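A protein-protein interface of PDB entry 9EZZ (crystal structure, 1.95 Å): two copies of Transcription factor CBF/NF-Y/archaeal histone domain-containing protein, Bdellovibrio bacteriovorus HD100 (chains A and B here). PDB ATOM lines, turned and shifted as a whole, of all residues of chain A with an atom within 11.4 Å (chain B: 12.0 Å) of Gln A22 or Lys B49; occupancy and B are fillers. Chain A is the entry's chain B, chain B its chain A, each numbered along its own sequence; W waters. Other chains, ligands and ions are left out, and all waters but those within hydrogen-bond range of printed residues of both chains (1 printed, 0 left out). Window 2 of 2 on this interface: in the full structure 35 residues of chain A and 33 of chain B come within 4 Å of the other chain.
Of the 14 printed residues of chain A, 10 touch a printed residue of chain B.
Printed residues of chain A that touch a printed residue of chain B: Val A13, Leu A16, Ile A17, Lys A20, Gly A21, Gln A22, Met A23, Asn A24, Thr A25 and Ser A26.
Among the printed residues, 20 pairs touch across the chains.
Water W1 lies within hydrogen-bond range of the side-chain amide oxygen of Gln A22 (2.5 Å), the side-chain amino group of Lys B49 (2.7 Å) and the backbone carbonyl oxygen of Gly A21 (3.2 Å).
OD2 of Asp B51 is in salt-bridge range of NE of Arg B53 (2.6 Å).
NH1 of Arg B53 sits at hydrogen-bond distance from O of Thr B55, at 2.9 Å.
NH1 of Arg B59 lies close to SD of Met B57 (3.5 Å).
The backbone NH (N) of Met B57 is in hydrogen-bond range of the side-chain carboxylate (OD2) of Asp B60.
The backbone carbonyl oxygen of Ile A17 sits at hydrogen-bond distance from the backbone NH of Gln A22 (3.5 Å).
O of Ile A17 sits at hydrogen-bond distance from N of Met A23 (3.5 Å).
CG1 of Val A13 touches SG of Cys B41, 3.8 Å away.
Ile A17 touches Cys B41 (CG1 to CB, 3.9 Å).
Val B56 touches Ile A17 (CG2 to CG2, 3.6 Å).
Gln A22 touches Lys B49.
SD of Met A23 touches CG of Lys B49, 3.9 Å away.
Met A23 touches Lys B54.
Asn A24 touches Thr B55 (O to CA, 3.3 Å).
CA of Thr A25 touches O of Val B56 (3.8 Å).
Ser A26 touches Thr B55.
Ala B58 touches Ser A26 (N to OG, 3.97 Å).
No position is printed for both chains.
Of the 20 pairs that touch across the chains among the printed residues, none has its exchanged pair printed and touching as well.
O of Lys B54 lies within hydrogen-bond range of N of Asn A24 (2.8 Å).
N of Val B56 sits at hydrogen-bond distance from O of Asn A24, at 2.9 Å.
The backbone NH (N) of Ser A26 lies within hydrogen-bond range of the backbone carbonyl oxygen (O) of Val B56 (3.0 Å).
The backbone carbonyl oxygen (O) of Arg B53 lies close to the side-chain sulfur (SD) of Met A23, at 3.3 Å.
No residue of chain B comes within 4 Å of Lys A18.
No residue of chain B comes within 4 Å of Glu A19.
Printed residues of chain B within 4 Å of Gly A21: Val B45 (3.7 Å).
Printed residues of chain B within 4 Å of Gln A22: Lys B49 (3.99 Å).
Of chain B, only Lys B54, Thr B55 and Val B56 come within 4 Å of Asn A24.
Of the printed residues of chain A, Leu B42 touches Lys A20.
Lys B43 touches none of the printed residues of chain A.
No residue of chain A comes within 4 Å of Ser B47.
Of the printed residues of chain A, Lys B49 touches Gln A22 and Met A23.
No residue of chain A comes within 4 Å of Ala B50.
No residue of chain A comes within 4 Å of Gly B52.
Printed residues of chain A within 4 Å of Lys B54: Met A23 and Asn A24.
Of the printed residues of chain A, Val B56 touches Ile A17 (3.6 Å), Asn A24 (2.9 Å), Thr A25 (3.8 Å) and Ser A26 (3.0 Å).
Of the printed residues of chain A, Met B57 touches Ser A26 (3.7 Å).
Ile B61 touches none of the printed residues of chain A.
The nearest printed residue of chain B that does not touch Gln A22 is Lys B54 (4.7 Å).
The nearest printed residue of chain A that does not touch Lys B49 is Gly A21 (4.2 Å).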
ATOM      1  N   VAL A  13      11.766  -0.031  21.686  1.00  0.00           N
ATOM      2  CA  VAL A  13      12.508  -0.049  22.978  1.00  0.00           C
ATOM      3  C   VAL A  13      13.455  -1.254  22.979  1.00  0.00           C
ATOM      4  O   VAL A  13      14.637  -1.080  23.359  1.00  0.00           O
ATOM      5  CB  VAL A  13      11.551  -0.093  24.187  1.00  0.00           C
ATOM      6  CG1 VAL A  13      12.285  -0.438  25.475  1.00  0.00           C
ATOM      7  CG2 VAL A  13      10.784   1.209  24.343  1.00  0.00           C
ATOM      8  N   LYS A  14      12.952  -2.428  22.590  1.00  0.00           N
ATOM      9  CA  LYS A  14      13.752  -3.673  22.564  1.00  0.00           C
ATOM     10  C   LYS A  14      14.871  -3.523  21.527  1.00  0.00           C
ATOM     11  O   LYS A  14      15.982  -3.992  21.818  1.00  0.00           O
ATOM     12  CB  LYS A  14      12.860  -4.884  22.296  1.00  0.00           C
ATOM     13  CG  LYS A  14      11.957  -5.287  23.458  1.00  0.00           C
ATOM     14  CD  LYS A  14      11.201  -6.576  23.175  1.00  0.00           C
ATOM     15  CE  LYS A  14      10.200  -6.976  24.239  1.00  0.00           C
ATOM     16  N   LYS A  15      14.611  -2.862  20.396  1.00  0.00           N
ATOM     17  CA  LYS A  15      15.598  -2.684  19.294  1.00  0.00           C
ATOM     18  C   LYS A  15      16.713  -1.749  19.763  1.00  0.00           C
ATOM     19  O   LYS A  15      17.887  -2.039  19.454  1.00  0.00           O
ATOM     20  CB  LYS A  15      14.935  -2.122  18.029  1.00  0.00           C
ATOM     21  CG  LYS A  15      15.790  -2.122  16.769  1.00  0.00           C
ATOM     22  CD  LYS A  15      15.249  -1.220  15.675  1.00  0.00           C
ATOM     23  N   LEU A  16      16.357  -0.663  20.453  1.00  0.00           N
ATOM     24  CA  LEU A  16      17.323   0.325  21.004  1.00  0.00           C
ATOM     25  C   LEU A  16      18.268  -0.387  21.981  1.00  0.00           C
ATOM     26  O   LEU A  16      19.492  -0.221  21.870  1.00  0.00           O
ATOM     27  CB  LEU A  16      16.548   1.425  21.728  1.00  0.00           C
ATOM     28  CG  LEU A  16      17.408   2.438  22.483  1.00  0.00           C
ATOM     29  CD1 LEU A  16      18.183   3.304  21.513  1.00  0.00           C
ATOM     30  CD2 LEU A  16      16.555   3.289  23.408  1.00  0.00           C
ATOM     31  N   ILE A  17      17.701  -1.147  22.915  1.00  0.00           N
ATOM     32  CA  ILE A  17      18.467  -1.845  23.988  1.00  0.00           C
ATOM     33  C   ILE A  17      19.322  -2.957  23.362  1.00  0.00           C
ATOM     34  O   ILE A  17      20.460  -3.156  23.830  1.00  0.00           O
ATOM     35  CB  ILE A  17      17.499  -2.344  25.077  1.00  0.00           C
ATOM     36  CG1 ILE A  17      16.950  -1.158  25.878  1.00  0.00           C
ATOM     37  CG2 ILE A  17      18.175  -3.389  25.951  1.00  0.00           C
ATOM     38  CD1 ILE A  17      15.909  -1.515  26.907  1.00  0.00           C
ATOM     39  N   LYS A  18      18.808  -3.650  22.340  1.00  0.00           N
ATOM     40  CA  LYS A  18      19.549  -4.708  21.606  1.00  0.00           C
ATOM     41  C   LYS A  18      20.684  -4.050  20.815  1.00  0.00           C
ATOM     42  O   LYS A  18      21.825  -4.528  20.927  1.00  0.00           O
ATOM     43  CB  LYS A  18      18.616  -5.506  20.686  1.00  0.00           C
ATOM     44  CG  LYS A  18      19.283  -6.593  19.841  1.00  0.00           C
ATOM     45  CD  LYS A  18      19.255  -7.974  20.477  1.00  0.00           C
ATOM     46  N   GLU A  19      20.390  -2.984  20.074  1.00  0.00           N
ATOM     47  CA  GLU A  19      21.361  -2.317  19.166  1.00  0.00           C
ATOM     48  C   GLU A  19      22.426  -1.592  20.000  1.00  0.00           C
ATOM     49  O   GLU A  19      23.612  -1.708  19.653  1.00  0.00           O
ATOM     50  CB  GLU A  19      20.651  -1.350  18.210  1.00  0.00           C
ATOM     51  N   LYS A  20      22.030  -0.866  21.052  1.00  0.00           N
ATOM     52  CA  LYS A  20      22.964   0.000  21.822  1.00  0.00           C
ATOM     53  C   LYS A  20      23.659  -0.804  22.931  1.00  0.00           C
ATOM     54  O   LYS A  20      24.785  -0.414  23.323  1.00  0.00           O
ATOM     55  CB  LYS A  20      22.242   1.233  22.372  1.00  0.00           C
ATOM     56  CG  LYS A  20      21.824   2.264  21.329  1.00  0.00           C
ATOM     57  CD  LYS A  20      23.004   2.851  20.564  1.00  0.00           C
ATOM     58  CE  LYS A  20      22.771   4.248  20.037  1.00  0.00           C
ATOM     59  NZ  LYS A  20      24.051   4.871  19.619  1.00  0.00           N
ATOM     60  N   GLY A  21      23.066  -1.908  23.399  1.00  0.00           N
ATOM     61  CA  GLY A  21      23.579  -2.639  24.577  1.00  0.00           C
ATOM     62  C   GLY A  21      23.938  -4.090  24.318  1.00  0.00           C
ATOM     63  O   GLY A  21      24.609  -4.668  25.196  1.00  0.00           O
ATOM     64  N   GLN A  22      23.531  -4.669  23.182  1.00  0.00           N
ATOM     65  CA  GLN A  22      23.529  -6.142  22.932  1.00  0.00           C
ATOM     66  C   GLN A  22      22.845  -6.844  24.112  1.00  0.00           C
ATOM     67  O   GLN A  22      23.358  -7.880  24.580  1.00  0.00           O
ATOM     68  CB  GLN A  22      24.932  -6.738  22.770  1.00  0.00           C
ATOM     69  CG  GLN A  22      25.826  -6.041  21.758  1.00  0.00           C
ATOM     70  CD  GLN A  22      26.462  -4.820  22.374  1.00  0.00           C
ATOM     71  OE1 GLN A  22      27.169  -4.892  23.385  1.00  0.00           O
ATOM     72  NE2 GLN A  22      26.198  -3.676  21.772  1.00  0.00           N
ATOM     73  N   MET A  23      21.718  -6.309  24.574  1.00  0.00           N
ATOM     74  CA  MET A  23      20.980  -6.843  25.753  1.00  0.00           C
ATOM     75  C   MET A  23      19.539  -7.148  25.343  1.00  0.00           C
ATOM     76  O   MET A  23      19.041  -6.488  24.415  1.00  0.00           O
ATOM     77  CB  MET A  23      20.935  -5.848  26.918  1.00  0.00           C
ATOM     78  CG  MET A  23      22.260  -5.276  27.336  1.00  0.00           C
ATOM     79  SD  MET A  23      23.139  -6.285  28.541  1.00  0.00           S
ATOM     80  CE  MET A  23      22.154  -5.984  30.000  1.00  0.00           C
ATOM     81  N   ASN A  24      18.931  -8.124  26.021  1.00  0.00           N
ATOM     82  CA  ASN A  24      17.477  -8.391  25.956  1.00  0.00           C
ATOM     83  C   ASN A  24      16.783  -7.418  26.907  1.00  0.00           C
ATOM     84  O   ASN A  24      17.477  -6.764  27.720  1.00  0.00           O
ATOM     85  CB  ASN A  24      17.118  -9.827  26.336  1.00  0.00           C
ATOM     86  CG  ASN A  24      17.860 -10.849  25.502  1.00  0.00           C
ATOM     87  OD1 ASN A  24      18.153 -10.621  24.332  1.00  0.00           O
ATOM     88  ND2 ASN A  24      18.186 -11.979  26.101  1.00  0.00           N
ATOM     89  N   THR A  25      15.458  -7.327  26.792  1.00  0.00           N
ATOM     90  CA  THR A  25      14.606  -6.466  27.638  1.00  0.00           C
ATOM     91  C   THR A  25      13.557  -7.354  28.297  1.00  0.00           C
ATOM     92  O   THR A  25      12.858  -8.060  27.567  1.00  0.00           O
ATOM     93  CB  THR A  25      13.931  -5.367  26.816  1.00  0.00           C
ATOM     94  OG1 THR A  25      14.926  -4.699  26.041  1.00  0.00           O
ATOM     95  CG2 THR A  25      13.186  -4.373  27.678  1.00  0.00           C
ATOM     96  N   SER A  26      13.453  -7.308  29.616  1.00  0.00           N
ATOM     97  CA  SER A  26      12.419  -8.036  30.396  1.00  0.00           C
ATOM     98  C   SER A  26      11.039  -7.411  30.146  1.00  0.00           C
ATOM     99  O   SER A  26      10.969  -6.216  29.864  1.00  0.00           O
ATOM    100  CB  SER A  26      12.774  -8.020  31.852  1.00  0.00           C
ATOM    101  OG  SER A  26      12.265  -6.842  32.469  1.00  0.00           O
ATOM    102  N   LEU B  40      16.293   6.656  29.863  1.00  0.00           N
ATOM    103  CA  LEU B  40      15.992   5.615  30.875  1.00  0.00           C
ATOM    104  C   LEU B  40      16.532   4.261  30.402  1.00  0.00           C
ATOM    105  O   LEU B  40      17.124   3.545  31.240  1.00  0.00           O
ATOM    106  CB  LEU B  40      14.487   5.556  31.145  1.00  0.00           C
ATOM    107  CG  LEU B  40      13.931   6.676  32.023  1.00  0.00           C
ATOM    108  CD1 LEU B  40      12.426   6.525  32.187  1.00  0.00           C
ATOM    109  CD2 LEU B  40      14.619   6.698  33.379  1.00  0.00           C
ATOM    110  N   CYS B  41      16.337   3.917  29.128  1.00  0.00           N
ATOM    111  CA  CYS B  41      16.797   2.631  28.543  1.00  0.00           C
ATOM    112  C   CYS B  41      18.324   2.542  28.558  1.00  0.00           C
ATOM    113  O   CYS B  41      18.844   1.458  28.848  1.00  0.00           O
ATOM    114  CB  CYS B  41      16.329   2.482  27.106  1.00  0.00           C
ATOM    115  SG  CYS B  41      14.553   2.177  27.014  1.00  0.00           S
ATOM    116  N   LEU B  42      19.007   3.634  28.214  1.00  0.00           N
ATOM    117  CA  LEU B  42      20.486   3.663  28.145  1.00  0.00           C
ATOM    118  C   LEU B  42      21.060   3.586  29.563  1.00  0.00           C
ATOM    119  O   LEU B  42      22.023   2.853  29.736  1.00  0.00           O
ATOM    120  CB  LEU B  42      20.937   4.914  27.392  1.00  0.00           C
ATOM    121  CG  LEU B  42      20.572   4.928  25.904  1.00  0.00           C
ATOM    122  CD1 LEU B  42      21.046   6.211  25.248  1.00  0.00           C
ATOM    123  CD2 LEU B  42      21.152   3.714  25.178  1.00  0.00           C
ATOM    124  N   LYS B  43      20.463   4.266  30.544  1.00  0.00           N
ATOM    125  CA  LYS B  43      20.873   4.124  31.967  1.00  0.00           C
ATOM    126  C   LYS B  43      20.624   2.675  32.395  1.00  0.00           C
ATOM    127  O   LYS B  43      21.447   2.134  33.131  1.00  0.00           O
ATOM    128  CB  LYS B  43      20.129   5.102  32.874  1.00  0.00           C
ATOM    129  CG  LYS B  43      20.606   6.543  32.791  1.00  0.00           C
ATOM    130  CD  LYS B  43      19.628   7.539  33.410  1.00  0.00           C
ATOM    131  CE  LYS B  43      20.245   8.367  34.520  1.00  0.00           C
ATOM    132  NZ  LYS B  43      21.112   9.439  33.978  1.00  0.00           N
ATOM    133  N   GLY B  44      19.542   2.075  31.911  1.00  0.00           N
ATOM    134  CA  GLY B  44      19.190   0.666  32.156  1.00  0.00           C
ATOM    135  C   GLY B  44      20.275  -0.275  31.667  1.00  0.00           C
ATOM    136  O   GLY B  44      20.693  -1.150  32.422  1.00  0.00           O
ATOM    137  N   VAL B  45      20.730  -0.087  30.437  1.00  0.00           N
ATOM    138  CA  VAL B  45      21.857  -0.868  29.847  1.00  0.00           C
ATOM    139  C   VAL B  45      23.080  -0.758  30.769  1.00  0.00           C
ATOM    140  O   VAL B  45      23.693  -1.800  31.056  1.00  0.00           O
ATOM    141  CB  VAL B  45      22.140  -0.420  28.402  1.00  0.00           C
ATOM    142  CG1 VAL B  45      23.458  -0.973  27.888  1.00  0.00           C
ATOM    143  CG2 VAL B  45      21.002  -0.802  27.468  1.00  0.00           C
ATOM    144  N   GLU B  46      23.411   0.443  31.253  1.00  0.00           N
ATOM    145  CA  GLU B  46      24.613   0.681  32.096  1.00  0.00           C
ATOM    146  C   GLU B  46      24.519  -0.177  33.362  1.00  0.00           C
ATOM    147  O   GLU B  46      25.488  -0.888  33.676  1.00  0.00           O
ATOM    148  CB  GLU B  46      24.726   2.146  32.518  1.00  0.00           C
ATOM    149  CG  GLU B  46      25.039   3.105  31.387  1.00  0.00           C
ATOM    150  CD  GLU B  46      26.338   2.796  30.666  1.00  0.00           C
ATOM    151  OE1 GLU B  46      27.426   3.177  31.196  1.00  0.00           O
ATOM    152  OE2 GLU B  46      26.259   2.148  29.602  1.00  0.00           O
ATOM    153  N   SER B  47      23.380  -0.101  34.064  1.00  0.00           N
ATOM    154  CA  SER B  47      23.132  -0.840  35.326  1.00  0.00           C
ATOM    155  C   SER B  47      23.255  -2.338  35.072  1.00  0.00           C
ATOM    156  O   SER B  47      23.954  -3.018  35.833  1.00  0.00           O
ATOM    157  CB  SER B  47      21.786  -0.492  35.903  1.00  0.00           C
ATOM    158  OG  SER B  47      21.786   0.866  36.313  1.00  0.00           O
ATOM    159  N   ALA B  48      22.600  -2.833  34.026  1.00  0.00           N
ATOM    160  CA  ALA B  48      22.548  -4.274  33.709  1.00  0.00           C
ATOM    161  C   ALA B  48      23.951  -4.788  33.394  1.00  0.00           C
ATOM    162  O   ALA B  48      24.342  -5.839  33.941  1.00  0.00           O
ATOM    163  CB  ALA B  48      21.589  -4.508  32.575  1.00  0.00           C
ATOM    164  N   LYS B  49      24.688  -4.040  32.563  1.00  0.00           N
ATOM    165  CA  LYS B  49      26.063  -4.394  32.156  1.00  0.00           C
ATOM    166  C   LYS B  49      26.971  -4.380  33.394  1.00  0.00           C
ATOM    167  O   LYS B  49      27.763  -5.326  33.542  1.00  0.00           O
ATOM    168  CB  LYS B  49      26.546  -3.455  31.048  1.00  0.00           C
ATOM    169  CG  LYS B  49      25.876  -3.715  29.705  1.00  0.00           C
ATOM    170  CD  LYS B  49      26.691  -3.285  28.511  1.00  0.00           C
ATOM    171  CE  LYS B  49      27.806  -4.242  28.177  1.00  0.00           C
ATOM    172  NZ  LYS B  49      28.529  -3.790  26.967  1.00  0.00           N
ATOM    173  N   ALA B  50      26.840  -3.369  34.255  1.00  0.00           N
ATOM    174  CA  ALA B  50      27.656  -3.229  35.482  1.00  0.00           C
ATOM    175  C   ALA B  50      27.425  -4.456  36.376  1.00  0.00           C
ATOM    176  O   ALA B  50      28.394  -4.892  37.022  1.00  0.00           O
ATOM    177  CB  ALA B  50      27.321  -1.938  36.184  1.00  0.00           C
ATOM    178  N   ASP B  51      26.204  -5.013  36.354  1.00  0.00           N
ATOM    179  CA  ASP B  51      25.786  -6.191  37.157  1.00  0.00           C
ATOM    180  C   ASP B  51      26.127  -7.500  36.432  1.00  0.00           C
ATOM    181  O   ASP B  51      25.747  -8.565  36.949  1.00  0.00           O
ATOM    182  CB  ASP B  51      24.288  -6.124  37.450  1.00  0.00           C
ATOM    183  CG  ASP B  51      23.833  -6.924  38.661  1.00  0.00           C
ATOM    184  OD1 ASP B  51      24.541  -6.905  39.686  1.00  0.00           O
ATOM    185  OD2 ASP B  51      22.773  -7.569  38.568  1.00  0.00           O
ATOM    186  N   GLY B  52      26.768  -7.432  35.266  1.00  0.00           N
ATOM    187  CA  GLY B  52      27.185  -8.608  34.478  1.00  0.00           C
ATOM    188  C   GLY B  52      26.016  -9.368  33.875  1.00  0.00           C
ATOM    189  O   GLY B  52      26.167 -10.581  33.685  1.00  0.00           O
ATOM    190  N   ARG B  53      24.891  -8.708  33.573  1.00  0.00           N
ATOM    191  CA  ARG B  53      23.672  -9.378  33.031  1.00  0.00           C
ATOM    192  C   ARG B  53      23.520  -9.094  31.531  1.00  0.00           C
ATOM    193  O   ARG B  53      24.179  -8.154  31.033  1.00  0.00           O
ATOM    194  CB  ARG B  53      22.418  -8.948  33.796  1.00  0.00           C
ATOM    195  CG  ARG B  53      22.278  -9.603  35.164  1.00  0.00           C
ATOM    196  CD  ARG B  53      21.053  -9.071  35.871  1.00  0.00           C
ATOM    197  NE  ARG B  53      21.204  -7.761  36.507  1.00  0.00           N
ATOM    198  CZ  ARG B  53      20.677  -6.609  36.085  1.00  0.00           C
ATOM    199  NH1 ARG B  53      19.978  -6.545  34.962  1.00  0.00           N
ATOM    200  NH2 ARG B  53      20.862  -5.507  36.797  1.00  0.00           N
ATOM    201  N   LYS B  54      22.700  -9.912  30.854  1.00  0.00           N
ATOM    202  CA  LYS B  54      22.402  -9.844  29.396  1.00  0.00           C
ATOM    203  C   LYS B  54      20.951  -9.382  29.186  1.00  0.00           C
ATOM    204  O   LYS B  54      20.499  -9.381  28.022  1.00  0.00           O
ATOM    205  CB  LYS B  54      22.613 -11.214  28.740  1.00  0.00           C
ATOM    206  CG  LYS B  54      24.034 -11.764  28.784  1.00  0.00           C
ATOM    207  N   THR B  55      20.254  -8.995  30.262  1.00  0.00           N
ATOM    208  CA  THR B  55      18.861  -8.487  30.236  1.00  0.00           C
ATOM    209  C   THR B  55      18.770  -7.202  31.058  1.00  0.00           C
ATOM    210  O   THR B  55      19.239  -7.186  32.217  1.00  0.00           O
ATOM    211  CB  THR B  55      17.864  -9.521  30.766  1.00  0.00           C
ATOM    212  OG1 THR B  55      18.092 -10.728  30.048  1.00  0.00           O
ATOM    213  CG2 THR B  55      16.418  -9.110  30.586  1.00  0.00           C
ATOM    214  N   VAL B  56      18.137  -6.178  30.480  1.00  0.00           N
ATOM    215  CA  VAL B  56      17.707  -4.967  31.215  1.00  0.00           C
ATOM    216  C   VAL B  56      16.423  -5.364  31.950  1.00  0.00           C
ATOM    217  O   VAL B  56      15.440  -5.791  31.302  1.00  0.00           O
ATOM    218  CB  VAL B  56      17.526  -3.759  30.284  1.00  0.00           C
ATOM    219  CG1 VAL B  56      17.093  -2.516  31.049  1.00  0.00           C
ATOM    220  CG2 VAL B  56      18.794  -3.470  29.490  1.00  0.00           C
ATOM    221  N   MET B  57      16.447  -5.255  33.272  1.00  0.00           N
ATOM    222  CA  MET B  57      15.319  -5.646  34.155  1.00  0.00           C
ATOM    223  C   MET B  57      14.701  -4.383  34.752  1.00  0.00           C
ATOM    224  O   MET B  57      15.287  -3.298  34.574  1.00  0.00           O
ATOM    225  CB  MET B  57      15.833  -6.556  35.267  1.00  0.00           C
ATOM    226  CG  MET B  57      16.349  -7.870  34.757  1.00  0.00           C
ATOM    227  SD  MET B  57      17.227  -8.669  36.099  1.00  0.00           S
ATOM    228  CE  MET B  57      15.836  -9.223  37.083  1.00  0.00           C
ATOM    229  N   ALA B  58      13.561  -4.520  35.421  1.00  0.00           N
ATOM    230  CA  ALA B  58      12.825  -3.378  35.997  1.00  0.00           C
ATOM    231  C   ALA B  58      13.738  -2.621  36.967  1.00  0.00           C
ATOM    232  O   ALA B  58      13.670  -1.384  36.959  1.00  0.00           O
ATOM    233  CB  ALA B  58      11.551  -3.852  36.655  1.00  0.00           C
ATOM    234  N   ARG B  59      14.583  -3.311  37.748  1.00  0.00           N
ATOM    235  CA  ARG B  59      15.398  -2.636  38.788  1.00  0.00           C
ATOM    236  C   ARG B  59      16.502  -1.803  38.124  1.00  0.00           C
ATOM    237  O   ARG B  59      17.061  -0.956  38.827  1.00  0.00           O
ATOM    238  CB  ARG B  59      15.964  -3.635  39.801  1.00  0.00           C
ATOM    239  CG  ARG B  59      16.943  -4.652  39.242  1.00  0.00           C
ATOM    240  CD  ARG B  59      17.644  -5.317  40.420  1.00  0.00           C
ATOM    241  NE  ARG B  59      18.768  -6.143  40.030  1.00  0.00           N
ATOM    242  CZ  ARG B  59      18.713  -7.425  39.655  1.00  0.00           C
ATOM    243  NH1 ARG B  59      17.557  -8.065  39.580  1.00  0.00           N
ATOM    244  NH2 ARG B  59      19.836  -8.052  39.334  1.00  0.00           N
ATOM    245  N   ASP B  60      16.754  -1.995  36.826  1.00  0.00           N
ATOM    246  CA  ASP B  60      17.737  -1.176  36.059  1.00  0.00           C
ATOM    247  C   ASP B  60      17.111   0.166  35.654  1.00  0.00           C
ATOM    248  O   ASP B  60      17.872   1.052  35.253  1.00  0.00           O
ATOM    249  CB  ASP B  60      18.239  -1.936  34.830  1.00  0.00           C
ATOM    250  CG  ASP B  60      18.970  -3.216  35.178  1.00  0.00           C
ATOM    251  OD1 ASP B  60      19.776  -3.181  36.116  1.00  0.00           O
ATOM    252  OD2 ASP B  60      18.720  -4.245  34.508  1.00  0.00           O
ATOM    253  N   ILE B  61      15.788   0.315  35.747  1.00  0.00           N
ATOM    254  CA  ILE B  61      15.071   1.546  35.302  1.00  0.00           C
ATOM    255  C   ILE B  61      14.757   2.367  36.548  1.00  0.00           C
ATOM    256  O   ILE B  61      13.780   2.053  37.251  1.00  0.00           O
ATOM    257  CB  ILE B  61      13.812   1.207  34.482  1.00  0.00           C
ATOM    258  CG1 ILE B  61      14.105   0.233  33.343  1.00  0.00           C
ATOM    259  CG2 ILE B  61      13.129   2.471  33.976  1.00  0.00           C
ATOM    260  CD1 ILE B  61      15.188   0.691  32.390  1.00  0.00           C
ATOM    261  N   VAL B  62      15.573   3.384  36.811  1.00  0.00           N
ATOM    262  CA  VAL B  62      15.503   4.175  38.071  1.00  0.00           C
ATOM    263  C   VAL B  62      14.696   5.446  37.786  1.00  0.00           C
ATOM    264  O   VAL B  62      15.115   6.224  36.920  1.00  0.00           O
ATOM    265  CB  VAL B  62      16.911   4.460  38.614  1.00  0.00           C
ATOM    266  CG1 VAL B  62      16.856   5.316  39.867  1.00  0.00           C
ATOM    267  CG2 VAL B  62      17.675   3.167  38.876  1.00  0.00           C
HETATM  268  O   HOH W   1      27.248  -2.856  24.828  1.00  0.00           O
